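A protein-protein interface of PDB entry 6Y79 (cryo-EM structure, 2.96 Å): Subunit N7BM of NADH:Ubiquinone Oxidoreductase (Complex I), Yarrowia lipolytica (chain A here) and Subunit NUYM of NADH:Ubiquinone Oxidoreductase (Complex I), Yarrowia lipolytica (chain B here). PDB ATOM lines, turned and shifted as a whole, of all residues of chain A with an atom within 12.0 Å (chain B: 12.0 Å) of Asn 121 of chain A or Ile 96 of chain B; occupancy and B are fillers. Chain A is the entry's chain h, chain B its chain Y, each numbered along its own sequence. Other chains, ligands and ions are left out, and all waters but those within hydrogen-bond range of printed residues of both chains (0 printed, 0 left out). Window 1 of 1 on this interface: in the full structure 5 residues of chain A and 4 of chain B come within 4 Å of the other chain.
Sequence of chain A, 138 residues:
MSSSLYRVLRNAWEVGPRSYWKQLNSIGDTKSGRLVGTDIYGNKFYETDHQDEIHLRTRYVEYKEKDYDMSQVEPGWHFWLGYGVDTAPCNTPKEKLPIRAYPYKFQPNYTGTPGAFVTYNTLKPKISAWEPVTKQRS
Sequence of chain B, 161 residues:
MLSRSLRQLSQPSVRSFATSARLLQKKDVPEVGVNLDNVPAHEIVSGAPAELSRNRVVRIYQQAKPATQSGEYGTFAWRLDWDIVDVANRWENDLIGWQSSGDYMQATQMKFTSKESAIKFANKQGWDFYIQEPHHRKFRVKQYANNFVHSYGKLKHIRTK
The backbone NH (N) of Lys 126 of chain A sits at hydrogen-bond distance from the side-chain carboxylate (OE1) of Glu 92 of chain B, 3.2 Å away. O of Leu 95 of chain B sits at hydrogen-bond distance from N of Asn 121 of chain A (3.2 Å). O of Ile 96 of chain B lies close to OD1 of Asn 121 of chain A (3.0 Å).
The side-chain amide oxygen of Asn 93 of chain B sits close to the backbone NH of Leu 95 of chain B. The backbone NH of Leu 123 of chain A is in hydrogen-bond range of the side-chain amide oxygen of Asn 121 of chain A (3.0 Å).
Among the printed residues, merely in contact across the chains: Thr 119 of chain A with Ile 96 of chain B (3.96 Å), Tyr 120 of chain A with Leu 95 of chain B (3.3 Å), Tyr 120 of chain A with Ile 96 of chain B (3.9 Å), Asn 121 of chain A with Gly 97 of chain B (3.8 Å) and Pro 125 of chain A with Glu 92 of chain B (3.9 Å).
Asn 121 of chain A touches just these residues of chain B: Leu 95, Ile 96 and Gly 97. Of chain B, only Ile 96 comes within 4 Å of Thr 119 of chain A. Tyr 120 of chain A touches just these residues of chain B: Leu 95 and Ile 96. No residue of chain B comes within 4 Å of Thr 122 of chain A. No residue of chain B comes within 4 Å of Leu 123 of chain A. Of chain B, only Glu 92 (3.9 Å) comes within 4 Å of Pro 125 of chain A. Asn 93 of chain B touches none of the printed residues of chain A. Leu 95 of chain B touches two residues of chain A. Gly 97 of chain B touches one residue of chain A. Of the printed residues of chain B, Lys 126 of chain A touches Glu 92. Printed residues of chain A within 4 Å of Glu 92 of chain B: Pro 125 and Lys 126. Val 118 of chain A touches none of the printed residues of chain B. The nearest residue of chain A that does not touch Ile 96 of chain B is Thr 122 of chain A (4.8 Å).
Along chain B the printed residues that touch a printed residue of chain A span positions 92 to 97. Printed residues of chain A that touch a printed residue of chain B: Thr 119, Tyr 120, Asn 121, Pro 125 and Lys 126. Among the printed residues, 8 pairs touch across the chains.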
ATOM      1  N   PHE A 117      13.968 -25.429 -27.418  1.00  0.00           N
ATOM      2  CA  PHE A 117      12.653 -24.839 -27.623  1.00  0.00           C
ATOM      3  C   PHE A 117      12.718 -23.318 -27.603  1.00  0.00           C
ATOM      4  O   PHE A 117      13.502 -22.727 -26.857  1.00  0.00           O
ATOM      5  CB  PHE A 117      11.692 -25.356 -26.549  1.00  0.00           C
ATOM      6  CG  PHE A 117      10.344 -24.723 -26.597  1.00  0.00           C
ATOM      7  CD1 PHE A 117       9.538 -24.884 -27.709  1.00  0.00           C
ATOM      8  CD2 PHE A 117       9.883 -23.962 -25.536  1.00  0.00           C
ATOM      9  CE1 PHE A 117       8.305 -24.295 -27.762  1.00  0.00           C
ATOM     10  CE2 PHE A 117       8.651 -23.376 -25.587  1.00  0.00           C
ATOM     11  CZ  PHE A 117       7.868 -23.534 -26.706  1.00  0.00           C
ATOM     12  N   VAL A 118      11.910 -22.678 -28.449  1.00  0.00           N
ATOM     13  CA  VAL A 118      11.791 -21.229 -28.436  1.00  0.00           C
ATOM     14  C   VAL A 118      10.381 -20.862 -28.013  1.00  0.00           C
ATOM     15  O   VAL A 118       9.413 -21.374 -28.582  1.00  0.00           O
ATOM     16  CB  VAL A 118      12.127 -20.631 -29.813  1.00  0.00           C
ATOM     17  CG1 VAL A 118      11.953 -19.110 -29.803  1.00  0.00           C
ATOM     18  CG2 VAL A 118      13.517 -20.998 -30.208  1.00  0.00           C
ATOM     19  N   THR A 119      10.259 -19.975 -27.024  1.00  0.00           N
ATOM     20  CA  THR A 119       8.931 -19.500 -26.687  1.00  0.00           C
ATOM     21  C   THR A 119       8.633 -18.218 -27.440  1.00  0.00           C
ATOM     22  O   THR A 119       9.529 -17.473 -27.827  1.00  0.00           O
ATOM     23  CB  THR A 119       8.758 -19.290 -25.190  1.00  0.00           C
ATOM     24  OG1 THR A 119       7.392 -18.970 -24.945  1.00  0.00           O
ATOM     25  CG2 THR A 119       9.612 -18.135 -24.664  1.00  0.00           C
ATOM     26  N   TYR A 120       7.347 -17.979 -27.656  1.00  0.00           N
ATOM     27  CA  TYR A 120       6.902 -16.819 -28.410  1.00  0.00           C
ATOM     28  C   TYR A 120       5.452 -16.527 -28.048  1.00  0.00           C
ATOM     29  O   TYR A 120       4.821 -17.256 -27.280  1.00  0.00           O
ATOM     30  CB  TYR A 120       7.064 -17.029 -29.919  1.00  0.00           C
ATOM     31  CG  TYR A 120       6.295 -18.202 -30.471  1.00  0.00           C
ATOM     32  CD1 TYR A 120       6.835 -19.478 -30.457  1.00  0.00           C
ATOM     33  CD2 TYR A 120       5.034 -18.033 -31.018  1.00  0.00           C
ATOM     34  CE1 TYR A 120       6.135 -20.548 -30.951  1.00  0.00           C
ATOM     35  CE2 TYR A 120       4.332 -19.095 -31.505  1.00  0.00           C
ATOM     36  CZ  TYR A 120       4.886 -20.349 -31.474  1.00  0.00           C
ATOM     37  OH  TYR A 120       4.184 -21.413 -31.973  1.00  0.00           O
ATOM     38  N   ASN A 121       4.927 -15.452 -28.624  1.00  0.00           N
ATOM     39  CA  ASN A 121       3.559 -15.030 -28.365  1.00  0.00           C
ATOM     40  C   ASN A 121       2.609 -15.807 -29.256  1.00  0.00           C
ATOM     41  O   ASN A 121       2.748 -15.798 -30.482  1.00  0.00           O
ATOM     42  CB  ASN A 121       3.409 -13.530 -28.616  1.00  0.00           C
ATOM     43  CG  ASN A 121       2.121 -12.948 -28.041  1.00  0.00           C
ATOM     44  OD1 ASN A 121       1.185 -13.664 -27.694  1.00  0.00           O
ATOM     45  ND2 ASN A 121       2.077 -11.632 -27.932  1.00  0.00           N
ATOM     46  N   THR A 122       1.619 -16.445 -28.641  1.00  0.00           N
ATOM     47  CA  THR A 122       0.687 -17.218 -29.431  1.00  0.00           C
ATOM     48  C   THR A 122      -0.280 -16.304 -30.167  1.00  0.00           C
ATOM     49  O   THR A 122      -0.791 -16.691 -31.210  1.00  0.00           O
ATOM     50  CB  THR A 122      -0.026 -18.213 -28.528  1.00  0.00           C
ATOM     51  OG1 THR A 122       0.921 -18.748 -27.612  1.00  0.00           O
ATOM     52  CG2 THR A 122      -0.656 -19.375 -29.343  1.00  0.00           C
ATOM     53  N   LEU A 123      -0.506 -15.083 -29.688  1.00  0.00           N
ATOM     54  CA  LEU A 123      -1.462 -14.192 -30.331  1.00  0.00           C
ATOM     55  C   LEU A 123      -0.833 -12.874 -30.773  1.00  0.00           C
ATOM     56  O   LEU A 123       0.312 -12.555 -30.461  1.00  0.00           O
ATOM     57  CB  LEU A 123      -2.667 -13.962 -29.426  1.00  0.00           C
ATOM     58  CG  LEU A 123      -2.598 -13.551 -27.971  1.00  0.00           C
ATOM     59  CD1 LEU A 123      -2.451 -12.076 -27.798  1.00  0.00           C
ATOM     60  CD2 LEU A 123      -3.917 -13.938 -27.469  1.00  0.00           C
ATOM     61  N   LYS A 124      -1.599 -12.135 -31.562  1.00  0.00           N
ATOM     62  CA  LYS A 124      -1.122 -10.919 -32.187  1.00  0.00           C
ATOM     63  C   LYS A 124      -1.277  -9.763 -31.205  1.00  0.00           C
ATOM     64  O   LYS A 124      -2.006  -9.904 -30.220  1.00  0.00           O
ATOM     65  CB  LYS A 124      -1.898 -10.689 -33.480  1.00  0.00           C
ATOM     66  CG  LYS A 124      -3.371 -10.543 -33.304  1.00  0.00           C
ATOM     67  CD  LYS A 124      -4.031 -10.340 -34.646  1.00  0.00           C
ATOM     68  CE  LYS A 124      -3.773 -11.522 -35.560  1.00  0.00           C
ATOM     69  NZ  LYS A 124      -4.684 -11.522 -36.727  1.00  0.00           N
ATOM     70  N   PRO A 125      -0.550  -8.640 -31.406  1.00  0.00           N
ATOM     71  CA  PRO A 125      -0.616  -7.522 -30.445  1.00  0.00           C
ATOM     72  C   PRO A 125      -2.025  -6.985 -30.230  1.00  0.00           C
ATOM     73  O   PRO A 125      -2.829  -6.905 -31.159  1.00  0.00           O
ATOM     74  CB  PRO A 125       0.293  -6.460 -31.079  1.00  0.00           C
ATOM     75  CG  PRO A 125       0.478  -6.913 -32.508  1.00  0.00           C
ATOM     76  CD  PRO A 125       0.537  -8.388 -32.371  1.00  0.00           C
ATOM     77  N   LYS A 126      -2.313  -6.645 -28.963  1.00  0.00           N
ATOM     78  CA  LYS A 126      -3.695  -6.549 -28.490  1.00  0.00           C
ATOM     79  C   LYS A 126      -4.438  -5.370 -29.094  1.00  0.00           C
ATOM     80  O   LYS A 126      -5.661  -5.429 -29.247  1.00  0.00           O
ATOM     81  CB  LYS A 126      -3.749  -6.446 -26.962  1.00  0.00           C
ATOM     82  CG  LYS A 126      -3.164  -7.626 -26.221  1.00  0.00           C
ATOM     83  CD  LYS A 126      -3.883  -8.909 -26.559  1.00  0.00           C
ATOM     84  CE  LYS A 126      -5.084  -9.132 -25.677  1.00  0.00           C
ATOM     85  NZ  LYS A 126      -5.861 -10.320 -26.118  1.00  0.00           N
ATOM     86  N   ILE A 127      -3.737  -4.298 -29.442  1.00  0.00           N
ATOM     87  CA  ILE A 127      -4.375  -3.101 -29.973  1.00  0.00           C
ATOM     88  C   ILE A 127      -3.824  -2.838 -31.365  1.00  0.00           C
ATOM     89  O   ILE A 127      -2.606  -2.719 -31.544  1.00  0.00           O
ATOM     90  CB  ILE A 127      -4.168  -1.885 -29.060  1.00  0.00           C
ATOM     91  CG1 ILE A 127      -4.894  -2.116 -27.737  1.00  0.00           C
ATOM     92  CG2 ILE A 127      -4.675  -0.625 -29.728  1.00  0.00           C
ATOM     93  CD1 ILE A 127      -4.893  -0.944 -26.817  1.00  0.00           C
ATOM     94  N   TRP B  91       1.960  -2.447 -20.260  1.00  0.00           N
ATOM     95  CA  TRP B  91       2.331  -2.665 -21.651  1.00  0.00           C
ATOM     96  C   TRP B  91       2.570  -4.147 -21.882  1.00  0.00           C
ATOM     97  O   TRP B  91       2.916  -4.882 -20.959  1.00  0.00           O
ATOM     98  CB  TRP B  91       3.573  -1.867 -22.057  1.00  0.00           C
ATOM     99  CG  TRP B  91       4.821  -2.192 -21.304  1.00  0.00           C
ATOM    100  CD1 TRP B  91       5.805  -3.045 -21.683  1.00  0.00           C
ATOM    101  CD2 TRP B  91       5.230  -1.636 -20.056  1.00  0.00           C
ATOM    102  NE1 TRP B  91       6.797  -3.068 -20.742  1.00  0.00           N
ATOM    103  CE2 TRP B  91       6.465  -2.212 -19.729  1.00  0.00           C
ATOM    104  CE3 TRP B  91       4.661  -0.721 -19.173  1.00  0.00           C
ATOM    105  CZ2 TRP B  91       7.143  -1.896 -18.566  1.00  0.00           C
ATOM    106  CZ3 TRP B  91       5.338  -0.410 -18.022  1.00  0.00           C
ATOM    107  CH2 TRP B  91       6.567  -0.991 -17.730  1.00  0.00           C
ATOM    108  N   GLU B  92       2.386  -4.577 -23.128  1.00  0.00           N
ATOM    109  CA  GLU B  92       2.531  -5.985 -23.469  1.00  0.00           C
ATOM    110  C   GLU B  92       3.982  -6.326 -23.772  1.00  0.00           C
ATOM    111  O   GLU B  92       4.721  -5.518 -24.336  1.00  0.00           O
ATOM    112  CB  GLU B  92       1.654  -6.347 -24.659  1.00  0.00           C
ATOM    113  CG  GLU B  92       1.585  -5.287 -25.727  1.00  0.00           C
ATOM    114  CD  GLU B  92       0.462  -5.553 -26.698  1.00  0.00           C
ATOM    115  OE1 GLU B  92      -0.096  -6.663 -26.643  1.00  0.00           O
ATOM    116  OE2 GLU B  92       0.142  -4.660 -27.508  1.00  0.00           O
ATOM    117  N   ASN B  93       4.374  -7.537 -23.411  1.00  0.00           N
ATOM    118  CA  ASN B  93       5.770  -7.937 -23.462  1.00  0.00           C
ATOM    119  C   ASN B  93       6.194  -8.250 -24.891  1.00  0.00           C
ATOM    120  O   ASN B  93       5.371  -8.649 -25.721  1.00  0.00           O
ATOM    121  CB  ASN B  93       5.982  -9.157 -22.561  1.00  0.00           C
ATOM    122  CG  ASN B  93       7.443  -9.484 -22.327  1.00  0.00           C
ATOM    123  OD1 ASN B  93       8.343  -8.778 -22.778  1.00  0.00           O
ATOM    124  ND2 ASN B  93       7.684 -10.572 -21.615  1.00  0.00           N
ATOM    125  N   ASP B  94       7.496  -8.030 -25.159  1.00  0.00           N
ATOM    126  CA  ASP B  94       8.183  -8.554 -26.339  1.00  0.00           C
ATOM    127  C   ASP B  94       7.832  -9.999 -26.604  1.00  0.00           C
ATOM    128  O   ASP B  94       7.492 -10.388 -27.723  1.00  0.00           O
ATOM    129  CB  ASP B  94       9.689  -8.574 -26.111  1.00  0.00           C
ATOM    130  CG  ASP B  94      10.387  -7.327 -26.537  1.00  0.00           C
ATOM    131  OD1 ASP B  94       9.794  -6.480 -27.235  1.00  0.00           O
ATOM    132  OD2 ASP B  94      11.553  -7.228 -26.150  1.00  0.00           O
ATOM    133  N   LEU B  95       7.947 -10.796 -25.568  1.00  0.00           N
ATOM    134  CA  LEU B  95       8.271 -12.201 -25.638  1.00  0.00           C
ATOM    135  C   LEU B  95       7.056 -13.093 -25.789  1.00  0.00           C
ATOM    136  O   LEU B  95       6.892 -13.785 -26.797  1.00  0.00           O
ATOM    137  CB  LEU B  95       9.009 -12.539 -24.364  1.00  0.00           C
ATOM    138  CG  LEU B  95       9.520 -13.938 -24.295  1.00  0.00           C
ATOM    139  CD1 LEU B  95      10.629 -14.050 -25.250  1.00  0.00           C
ATOM    140  CD2 LEU B  95      10.014 -14.067 -22.932  1.00  0.00           C
ATOM    141  N   ILE B  96       6.208 -13.076 -24.762  1.00  0.00           N
ATOM    142  CA  ILE B  96       4.994 -13.867 -24.720  1.00  0.00           C
ATOM    143  C   ILE B  96       3.756 -12.984 -24.706  1.00  0.00           C
ATOM    144  O   ILE B  96       2.680 -13.412 -25.118  1.00  0.00           O
ATOM    145  CB  ILE B  96       4.998 -14.814 -23.506  1.00  0.00           C
ATOM    146  CG1 ILE B  96       6.345 -15.491 -23.363  1.00  0.00           C
ATOM    147  CG2 ILE B  96       4.032 -15.943 -23.703  1.00  0.00           C
ATOM    148  CD1 ILE B  96       6.467 -16.320 -22.136  1.00  0.00           C
ATOM    149  N   GLY B  97       3.882 -11.743 -24.268  1.00  0.00           N
ATOM    150  CA  GLY B  97       2.718 -10.889 -24.272  1.00  0.00           C
ATOM    151  C   GLY B  97       2.129 -10.803 -22.890  1.00  0.00           C
ATOM    152  O   GLY B  97       0.921 -10.622 -22.715  1.00  0.00           O
ATOM    153  N   TRP B  98       2.991 -10.980 -21.901  1.00  0.00           N
ATOM    154  CA  TRP B  98       2.617 -10.719 -20.528  1.00  0.00           C
ATOM    155  C   TRP B  98       2.352  -9.238 -20.338  1.00  0.00           C
ATOM    156  O   TRP B  98       3.030  -8.389 -20.915  1.00  0.00           O
ATOM    157  CB  TRP B  98       3.722 -11.153 -19.584  1.00  0.00           C
ATOM    158  CG  TRP B  98       3.865 -12.606 -19.449  1.00  0.00           C
ATOM    159  CD1 TRP B  98       3.010 -13.563 -19.891  1.00  0.00           C
ATOM    160  CD2 TRP B  98       4.940 -13.285 -18.816  1.00  0.00           C
ATOM    161  NE1 TRP B  98       3.491 -14.803 -19.573  1.00  0.00           N
ATOM    162  CE2 TRP B  98       4.678 -14.655 -18.908  1.00  0.00           C
ATOM    163  CE3 TRP B  98       6.106 -12.862 -18.180  1.00  0.00           C
ATOM    164  CZ2 TRP B  98       5.536 -15.606 -18.388  1.00  0.00           C
ATOM    165  CZ3 TRP B  98       6.952 -13.801 -17.667  1.00  0.00           C
ATOM    166  CH2 TRP B  98       6.667 -15.158 -17.771  1.00  0.00           C
ATOM    167  N   GLN B  99       1.353  -8.934 -19.533  1.00  0.00           N
ATOM    168  CA  GLN B  99       1.073  -7.563 -19.147  1.00  0.00           C
ATOM    169  C   GLN B  99       2.119  -7.135 -18.130  1.00  0.00           C
ATOM    170  O   GLN B  99       2.066  -7.531 -16.968  1.00  0.00           O
ATOM    171  CB  GLN B  99      -0.333  -7.482 -18.581  1.00  0.00           C
ATOM    172  CG  GLN B  99      -1.366  -7.977 -19.547  1.00  0.00           C
ATOM    173  CD  GLN B  99      -1.538  -7.014 -20.663  1.00  0.00           C
ATOM    174  OE1 GLN B  99      -1.494  -5.812 -20.445  1.00  0.00           O
ATOM    175  NE2 GLN B  99      -1.739  -7.518 -21.866  1.00  0.00           N
ATOM    176  N   SER B 100       3.084  -6.336 -18.572  1.00  0.00           N
ATOM    177  CA  SER B 100       4.149  -5.813 -17.728  1.00  0.00           C
ATOM    178  C   SER B 100       3.762  -4.439 -17.213  1.00  0.00           C
ATOM    179  O   SER B 100       3.022  -3.710 -17.864  1.00  0.00           O
ATOM    180  CB  SER B 100       5.455  -5.700 -18.503  1.00  0.00           C
ATOM    181  OG  SER B 100       5.856  -6.954 -19.001  1.00  0.00           O
